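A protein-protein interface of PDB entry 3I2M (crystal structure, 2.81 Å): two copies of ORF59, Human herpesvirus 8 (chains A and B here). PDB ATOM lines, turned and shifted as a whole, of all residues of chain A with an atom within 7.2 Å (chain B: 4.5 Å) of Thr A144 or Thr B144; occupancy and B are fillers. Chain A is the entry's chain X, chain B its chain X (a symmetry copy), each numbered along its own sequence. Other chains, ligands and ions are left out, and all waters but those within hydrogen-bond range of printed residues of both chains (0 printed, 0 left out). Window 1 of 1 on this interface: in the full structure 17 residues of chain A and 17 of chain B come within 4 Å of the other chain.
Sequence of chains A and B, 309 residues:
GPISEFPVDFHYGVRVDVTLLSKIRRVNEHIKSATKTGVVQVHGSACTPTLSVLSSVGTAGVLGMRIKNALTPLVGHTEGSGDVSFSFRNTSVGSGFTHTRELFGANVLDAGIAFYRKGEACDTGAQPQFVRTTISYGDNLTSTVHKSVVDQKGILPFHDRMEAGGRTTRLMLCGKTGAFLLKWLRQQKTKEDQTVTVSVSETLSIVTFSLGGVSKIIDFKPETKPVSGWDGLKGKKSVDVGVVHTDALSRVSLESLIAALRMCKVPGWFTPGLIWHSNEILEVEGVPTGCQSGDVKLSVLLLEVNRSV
The backbone carbonyl oxygen of Ser B143 lies within hydrogen-bond range of the backbone NH of Lys A147 (3.0 Å).
N of Val A145 sits at hydrogen-bond distance from O of Val B145.
The side-chain hydroxyl (OG1) of Thr A144 is in hydrogen-bond range of the side-chain hydroxyl (OH) of Tyr A137 (3.4 Å).
N of Ile B135 sits at hydrogen-bond distance from O of Thr B144 (2.9 Å).
The side-chain hydroxyl (OH) of Tyr B137 lies within hydrogen-bond range of the side-chain hydroxyl (OG1) of Thr B144, 3.4 Å away.
N of Ile A135 lies within hydrogen-bond range of O of Thr A144 (2.9 Å).
OG of Ser A95 lies within hydrogen-bond range of NE2 of His A146 (3.4 Å).
The backbone carbonyl oxygen of Thr A133 is in hydrogen-bond range of the backbone NH of His A146.
Among the printed residues, pairs that only touch across the chains: Ser A95 with Tyr B137 (3.6 Å), Thr A142 with His B146 (3.4 Å), Ser A143 with Val B145 (3.9 Å), Ser A143 with His B146 (3.3 Å), Thr A144 with Thr B144 (3.7 Å), Thr A144 with Val B145 (3.7 Å), Thr A144 with His B146 (2.9 Å), Val A145 with Ser B143 (3.9 Å), Val A145 with Thr B144 (3.7 Å), His A146 with Ser B143 (3.3 Å) and His A146 with Thr B144 (2.9 Å).
Thr A133 touches none of the printed residues of chain B.
Of the printed residues of chain B, Ser A143 touches Val B145 (3.9 Å) and His B146 (3.3 Å).
Thr A144 touches three residues of chain B.
Of the printed residues of chain B, His A146 touches Ser B143 and Thr B144.
Ile B135 touches none of the printed residues of chain A.
Of the printed residues of chain A, Tyr B137 touches Ser A95.
Of the printed residues of chain A, Thr B144 touches Thr A144, Val A145 and His A146.
Printed residues of chain A that touch a printed residue of chain B: Ser A95, Thr A142, Ser A143, Thr A144, Val A145, His A146 and Lys A147.
Hydrophobic or aromatic side chains of chain A within 4 Å of the printed part of chain B: His A146.
Printed residues of chain B that touch a printed residue of chain A: Tyr B137, Ser B143, Thr B144, Val B145 and His B146.
Hydrophobic or aromatic side chains of chain B within 4 Å of the printed part of chain A: Tyr B137 and His B146.
Among the printed residues, 13 pairs touch across the chains.
Among the printed residues, no Asp or Glu carboxylate lies within 4 Å of a Lys or Arg side-chain nitrogen of the other chain.
Ser A143 touches Val B145, and with the chains exchanged Val A145 touches Ser B143.
Ser A143 touches His B146, and with the chains exchanged His A146 touches Ser B143.
Thr A144 touches its own counterpart, Thr B144.
Thr A144 touches His B146, and with the chains exchanged His A146 touches Thr B144.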
ATOM      1  N   SER A  95      10.249  -0.926  -3.306  1.00  0.00           N
ATOM      2  CA  SER A  95       9.629  -0.624  -4.607  1.00  0.00           C
ATOM      3  C   SER A  95       9.190   0.798  -4.797  1.00  0.00           C
ATOM      4  O   SER A  95       9.120   1.600  -3.855  1.00  0.00           O
ATOM      5  CB  SER A  95       8.362  -1.463  -4.866  1.00  0.00           C
ATOM      6  OG  SER A  95       8.664  -2.806  -5.136  1.00  0.00           O
ATOM      7  N   GLY A  96       8.892   1.070  -6.065  1.00  0.00           N
ATOM      8  CA  GLY A  96       8.394   2.346  -6.505  1.00  0.00           C
ATOM      9  C   GLY A  96       6.926   2.119  -6.817  1.00  0.00           C
ATOM     10  O   GLY A  96       6.224   3.057  -7.226  1.00  0.00           O
ATOM     11  N   PHE A  97       6.450   0.882  -6.631  1.00  0.00           N
ATOM     12  CA  PHE A  97       5.060   0.594  -6.907  1.00  0.00           C
ATOM     13  C   PHE A  97       4.165   0.764  -5.685  1.00  0.00           C
ATOM     14  O   PHE A  97       4.361   0.119  -4.653  1.00  0.00           O
ATOM     15  CB  PHE A  97       4.908  -0.795  -7.468  1.00  0.00           C
ATOM     16  CG  PHE A  97       3.520  -1.095  -7.949  1.00  0.00           C
ATOM     17  CD1 PHE A  97       3.163  -0.848  -9.277  1.00  0.00           C
ATOM     18  CD2 PHE A  97       2.560  -1.623  -7.084  1.00  0.00           C
ATOM     19  CE1 PHE A  97       1.881  -1.124  -9.723  1.00  0.00           C
ATOM     20  CE2 PHE A  97       1.275  -1.902  -7.529  1.00  0.00           C
ATOM     21  CZ  PHE A  97       0.937  -1.654  -8.841  1.00  0.00           C
ATOM     22  N   GLU A 102      -1.455   3.761  -8.228  1.00  0.00           N
ATOM     23  CA  GLU A 102      -1.756   3.237  -9.542  1.00  0.00           C
ATOM     24  C   GLU A 102      -3.220   2.959  -9.756  1.00  0.00           C
ATOM     25  O   GLU A 102      -3.740   3.268 -10.831  1.00  0.00           O
ATOM     26  CB  GLU A 102      -0.937   1.980  -9.812  1.00  0.00           C
ATOM     27  CG  GLU A 102       0.562   2.187  -9.667  1.00  0.00           C
ATOM     28  CD  GLU A 102       1.152   3.203 -10.643  1.00  0.00           C
ATOM     29  OE1 GLU A 102       0.702   3.282 -11.818  1.00  0.00           O
ATOM     30  OE2 GLU A 102       2.084   3.926 -10.222  1.00  0.00           O
ATOM     31  N   THR A 133      -1.036  -7.382  -9.010  1.00  0.00           N
ATOM     32  CA  THR A 133      -1.817  -6.246  -9.455  1.00  0.00           C
ATOM     33  C   THR A 133      -1.418  -5.911 -10.881  1.00  0.00           C
ATOM     34  O   THR A 133      -0.230  -5.840 -11.203  1.00  0.00           O
ATOM     35  CB  THR A 133      -1.607  -5.067  -8.509  1.00  0.00           C
ATOM     36  OG1 THR A 133      -2.038  -5.455  -7.198  1.00  0.00           O
ATOM     37  CG2 THR A 133      -2.390  -3.833  -8.969  1.00  0.00           C
ATOM     38  N   THR A 134      -2.414  -5.709 -11.731  1.00  0.00           N
ATOM     39  CA  THR A 134      -2.188  -5.405 -13.133  1.00  0.00           C
ATOM     40  C   THR A 134      -2.824  -4.092 -13.493  1.00  0.00           C
ATOM     41  O   THR A 134      -4.009  -3.882 -13.219  1.00  0.00           O
ATOM     42  CB  THR A 134      -2.801  -6.490 -13.993  1.00  0.00           C
ATOM     43  OG1 THR A 134      -2.159  -7.719 -13.666  1.00  0.00           O
ATOM     44  CG2 THR A 134      -2.610  -6.207 -15.479  1.00  0.00           C
ATOM     45  N   ILE A 135      -2.039  -3.210 -14.107  1.00  0.00           N
ATOM     46  CA  ILE A 135      -2.522  -1.899 -14.507  1.00  0.00           C
ATOM     47  C   ILE A 135      -2.383  -1.744 -16.032  1.00  0.00           C
ATOM     48  O   ILE A 135      -1.367  -2.138 -16.600  1.00  0.00           O
ATOM     49  CB  ILE A 135      -1.717  -0.778 -13.801  1.00  0.00           C
ATOM     50  CG1 ILE A 135      -1.576  -1.017 -12.286  1.00  0.00           C
ATOM     51  CG2 ILE A 135      -2.339   0.585 -14.074  1.00  0.00           C
ATOM     52  CD1 ILE A 135      -2.881  -0.988 -11.490  1.00  0.00           C
ATOM     53  N   SER A 136      -3.396  -1.176 -16.691  1.00  0.00           N
ATOM     54  CA  SER A 136      -3.363  -0.947 -18.132  1.00  0.00           C
ATOM     55  C   SER A 136      -3.667   0.511 -18.362  1.00  0.00           C
ATOM     56  O   SER A 136      -4.705   0.997 -17.945  1.00  0.00           O
ATOM     57  CB  SER A 136      -4.352  -1.843 -18.862  1.00  0.00           C
ATOM     58  OG  SER A 136      -3.968  -3.203 -18.748  1.00  0.00           O
ATOM     59  N   TYR A 137      -2.756   1.205 -19.031  1.00  0.00           N
ATOM     60  CA  TYR A 137      -2.877   2.639 -19.267  1.00  0.00           C
ATOM     61  C   TYR A 137      -3.602   3.121 -20.546  1.00  0.00           C
ATOM     62  O   TYR A 137      -4.034   2.313 -21.365  1.00  0.00           O
ATOM     63  CB  TYR A 137      -1.479   3.242 -19.145  1.00  0.00           C
ATOM     64  CG  TYR A 137      -0.838   2.916 -17.812  1.00  0.00           C
ATOM     65  CD1 TYR A 137      -1.065   3.706 -16.701  1.00  0.00           C
ATOM     66  CD2 TYR A 137      -0.007   1.815 -17.670  1.00  0.00           C
ATOM     67  CE1 TYR A 137      -0.486   3.414 -15.487  1.00  0.00           C
ATOM     68  CE2 TYR A 137       0.582   1.509 -16.462  1.00  0.00           C
ATOM     69  CZ  TYR A 137       0.344   2.306 -15.361  1.00  0.00           C
ATOM     70  OH  TYR A 137       0.938   2.002 -14.120  1.00  0.00           O
ATOM     71  N   THR A 142       0.680   0.444 -22.978  1.00  0.00           N
ATOM     72  CA  THR A 142       1.480   0.379 -21.753  1.00  0.00           C
ATOM     73  C   THR A 142       0.759  -0.348 -20.609  1.00  0.00           C
ATOM     74  O   THR A 142      -0.466  -0.302 -20.522  1.00  0.00           O
ATOM     75  CB  THR A 142       1.822   1.812 -21.279  1.00  0.00           C
ATOM     76  OG1 THR A 142       2.471   2.522 -22.336  1.00  0.00           O
ATOM     77  CG2 THR A 142       2.723   1.808 -20.055  1.00  0.00           C
ATOM     78  N   SER A 143       1.528  -1.014 -19.743  1.00  0.00           N
ATOM     79  CA  SER A 143       1.003  -1.725 -18.588  1.00  0.00           C
ATOM     80  C   SER A 143       2.109  -2.095 -17.581  1.00  0.00           C
ATOM     81  O   SER A 143       3.288  -2.220 -17.951  1.00  0.00           O
ATOM     82  CB  SER A 143       0.292  -3.000 -18.999  1.00  0.00           C
ATOM     83  OG  SER A 143       1.212  -3.951 -19.488  1.00  0.00           O
ATOM     84  N   THR A 144       1.714  -2.264 -16.315  1.00  0.00           N
ATOM     85  CA  THR A 144       2.622  -2.645 -15.256  1.00  0.00           C
ATOM     86  C   THR A 144       1.998  -3.808 -14.493  1.00  0.00           C
ATOM     87  O   THR A 144       0.800  -3.788 -14.213  1.00  0.00           O
ATOM     88  CB  THR A 144       2.806  -1.517 -14.249  1.00  0.00           C
ATOM     89  OG1 THR A 144       3.226  -0.314 -14.912  1.00  0.00           O
ATOM     90  CG2 THR A 144       3.840  -1.898 -13.192  1.00  0.00           C
ATOM     91  N   VAL A 145       2.801  -4.820 -14.156  1.00  0.00           N
ATOM     92  CA  VAL A 145       2.321  -5.985 -13.395  1.00  0.00           C
ATOM     93  C   VAL A 145       3.162  -6.148 -12.122  1.00  0.00           C
ATOM     94  O   VAL A 145       4.277  -6.673 -12.181  1.00  0.00           O
ATOM     95  CB  VAL A 145       2.397  -7.275 -14.237  1.00  0.00           C
ATOM     96  CG1 VAL A 145       1.945  -8.475 -13.420  1.00  0.00           C
ATOM     97  CG2 VAL A 145       1.543  -7.143 -15.479  1.00  0.00           C
ATOM     98  N   HIS A 146       2.652  -5.707 -10.974  1.00  0.00           N
ATOM     99  CA  HIS A 146       3.446  -5.820  -9.738  1.00  0.00           C
ATOM    100  C   HIS A 146       3.078  -7.121  -9.063  1.00  0.00           C
ATOM    101  O   HIS A 146       1.986  -7.645  -9.302  1.00  0.00           O
ATOM    102  CB  HIS A 146       3.298  -4.602  -8.838  1.00  0.00           C
ATOM    103  CG  HIS A 146       4.258  -4.573  -7.692  1.00  0.00           C
ATOM    104  ND1 HIS A 146       3.856  -4.615  -6.374  1.00  0.00           N
ATOM    105  CD2 HIS A 146       5.609  -4.506  -7.668  1.00  0.00           C
ATOM    106  CE1 HIS A 146       4.918  -4.572  -5.588  1.00  0.00           C
ATOM    107  NE2 HIS A 146       5.995  -4.507  -6.348  1.00  0.00           N
ATOM    108  N   LYS A 147       3.965  -7.650  -8.224  1.00  0.00           N
ATOM    109  CA  LYS A 147       3.675  -8.940  -7.655  1.00  0.00           C
ATOM    110  C   LYS A 147       4.362  -8.972  -6.313  1.00  0.00           C
ATOM    111  O   LYS A 147       5.594  -8.830  -6.235  1.00  0.00           O
ATOM    112  CB  LYS A 147       4.295  -9.934  -8.620  1.00  0.00           C
ATOM    113  CG  LYS A 147       3.544 -11.202  -8.880  1.00  0.00           C
ATOM    114  CD  LYS A 147       4.038 -11.761 -10.256  1.00  0.00           C
ATOM    115  CE  LYS A 147       3.126 -12.836 -10.872  1.00  0.00           C
ATOM    116  NZ  LYS A 147       3.540 -13.230 -12.260  1.00  0.00           N
ATOM    117  N   PHE B  97       6.164   4.225 -13.234  1.00  0.00           N
ATOM    118  CA  PHE B  97       7.368   3.463 -13.482  1.00  0.00           C
ATOM    119  C   PHE B  97       8.435   4.264 -14.221  1.00  0.00           C
ATOM    120  O   PHE B  97       8.212   4.759 -15.328  1.00  0.00           O
ATOM    121  CB  PHE B  97       7.050   2.203 -14.242  1.00  0.00           C
ATOM    122  CG  PHE B  97       8.221   1.276 -14.373  1.00  0.00           C
ATOM    123  CD1 PHE B  97       8.445   0.280 -13.418  1.00  0.00           C
ATOM    124  CD2 PHE B  97       9.107   1.387 -15.447  1.00  0.00           C
ATOM    125  CE1 PHE B  97       9.526  -0.577 -13.539  1.00  0.00           C
ATOM    126  CE2 PHE B  97      10.190   0.527 -15.570  1.00  0.00           C
ATOM    127  CZ  PHE B  97      10.399  -0.450 -14.620  1.00  0.00           C
ATOM    128  N   THR B 133      10.664  -4.348 -19.253  1.00  0.00           N
ATOM    129  CA  THR B 133      11.660  -4.272 -18.204  1.00  0.00           C
ATOM    130  C   THR B 133      11.176  -5.085 -17.016  1.00  0.00           C
ATOM    131  O   THR B 133      10.022  -4.967 -16.599  1.00  0.00           O
ATOM    132  CB  THR B 133      11.918  -2.815 -17.834  1.00  0.00           C
ATOM    133  OG1 THR B 133      12.401  -2.131 -18.998  1.00  0.00           O
ATOM    134  CG2 THR B 133      12.941  -2.697 -16.700  1.00  0.00           C
ATOM    135  N   THR B 134      12.062  -5.910 -16.476  1.00  0.00           N
ATOM    136  CA  THR B 134      11.738  -6.769 -15.350  1.00  0.00           C
ATOM    137  C   THR B 134      12.656  -6.486 -14.195  1.00  0.00           C
ATOM    138  O   THR B 134      13.879  -6.484 -14.363  1.00  0.00           O
ATOM    139  CB  THR B 134      11.902  -8.219 -15.755  1.00  0.00           C
ATOM    140  OG1 THR B 134      10.996  -8.478 -16.824  1.00  0.00           O
ATOM    141  CG2 THR B 134      11.593  -9.164 -14.599  1.00  0.00           C
ATOM    142  N   ILE B 135      12.070  -6.252 -13.025  1.00  0.00           N
ATOM    143  CA  ILE B 135      12.837  -5.960 -11.824  1.00  0.00           C
ATOM    144  C   ILE B 135      12.537  -7.023 -10.752  1.00  0.00           C
ATOM    145  O   ILE B 135      11.383  -7.405 -10.571  1.00  0.00           O
ATOM    146  CB  ILE B 135      12.480  -4.556 -11.272  1.00  0.00           C
ATOM    147  CG1 ILE B 135      12.489  -3.472 -12.365  1.00  0.00           C
ATOM    148  CG2 ILE B 135      13.411  -4.175 -10.129  1.00  0.00           C
ATOM    149  CD1 ILE B 135      13.848  -3.197 -13.009  1.00  0.00           C
ATOM    150  N   TYR B 137      13.294  -7.803  -6.672  1.00  0.00           N
ATOM    151  CA  TYR B 137      13.774  -7.215  -5.428  1.00  0.00           C
ATOM    152  C   TYR B 137      14.421  -8.142  -4.370  1.00  0.00           C
ATOM    153  O   TYR B 137      14.494  -9.354  -4.558  1.00  0.00           O
ATOM    154  CB  TYR B 137      12.629  -6.393  -4.840  1.00  0.00           C
ATOM    155  CG  TYR B 137      12.114  -5.361  -5.820  1.00  0.00           C
ATOM    156  CD1 TYR B 137      12.701  -4.113  -5.915  1.00  0.00           C
ATOM    157  CD2 TYR B 137      11.037  -5.638  -6.649  1.00  0.00           C
ATOM    158  CE1 TYR B 137      12.238  -3.173  -6.805  1.00  0.00           C
ATOM    159  CE2 TYR B 137      10.560  -4.707  -7.545  1.00  0.00           C
ATOM    160  CZ  TYR B 137      11.158  -3.466  -7.631  1.00  0.00           C
ATOM    161  OH  TYR B 137      10.681  -2.506  -8.544  1.00  0.00           O
ATOM    162  N   SER B 143       8.507  -8.421  -7.374  1.00  0.00           N
ATOM    163  CA  SER B 143       8.970  -8.064  -8.707  1.00  0.00           C
ATOM    164  C   SER B 143       7.955  -7.182  -9.457  1.00  0.00           C
ATOM    165  O   SER B 143       6.747  -7.214  -9.166  1.00  0.00           O
ATOM    166  CB  SER B 143       9.236  -9.299  -9.547  1.00  0.00           C
ATOM    167  OG  SER B 143       8.030  -9.960  -9.862  1.00  0.00           O
ATOM    168  N   THR B 144       8.459  -6.401 -10.418  1.00  0.00           N
ATOM    169  CA  THR B 144       7.636  -5.538 -11.237  1.00  0.00           C
ATOM    170  C   THR B 144       8.012  -5.771 -12.696  1.00  0.00           C
ATOM    171  O   THR B 144       9.196  -5.873 -13.017  1.00  0.00           O
ATOM    172  CB  THR B 144       7.913  -4.068 -10.949  1.00  0.00           C
ATOM    173  OG1 THR B 144       7.754  -3.792  -9.548  1.00  0.00           O
ATOM    174  CG2 THR B 144       6.970  -3.173 -11.750  1.00  0.00           C
ATOM    175  N   VAL B 145       7.015  -5.853 -13.579  1.00  0.00           N
ATOM    176  CA  VAL B 145       7.253  -6.050 -15.019  1.00  0.00           C
ATOM    177  C   VAL B 145       6.585  -4.916 -15.808  1.00  0.00           C
ATOM    178  O   VAL B 145       5.371  -4.949 -16.027  1.00  0.00           O
ATOM    179  CB  VAL B 145       6.707  -7.410 -15.499  1.00  0.00           C
ATOM    180  CG1 VAL B 145       6.918  -7.574 -16.995  1.00  0.00           C
ATOM    181  CG2 VAL B 145       7.385  -8.540 -14.755  1.00  0.00           C
ATOM    182  N   HIS B 146       7.350  -3.916 -16.237  1.00  0.00           N
ATOM    183  CA  HIS B 146       6.734  -2.796 -16.972  1.00  0.00           C
ATOM    184  C   HIS B 146       6.818  -3.103 -18.448  1.00  0.00           C
ATOM    185  O   HIS B 146       7.678  -3.887 -18.862  1.00  0.00           O
ATOM    186  CB  HIS B 146       7.337  -1.451 -16.594  1.00  0.00           C
ATOM    187  CG  HIS B 146       6.591  -0.276 -17.138  1.00  0.00           C
ATOM    188  ND1 HIS B 146       7.144   0.616 -18.034  1.00  0.00           N
ATOM    189  CD2 HIS B 146       5.328   0.155 -16.915  1.00  0.00           C
ATOM    190  CE1 HIS B 146       6.254   1.547 -18.334  1.00  0.00           C
ATOM    191  NE2 HIS B 146       5.143   1.290 -17.669  1.00  0.00           N
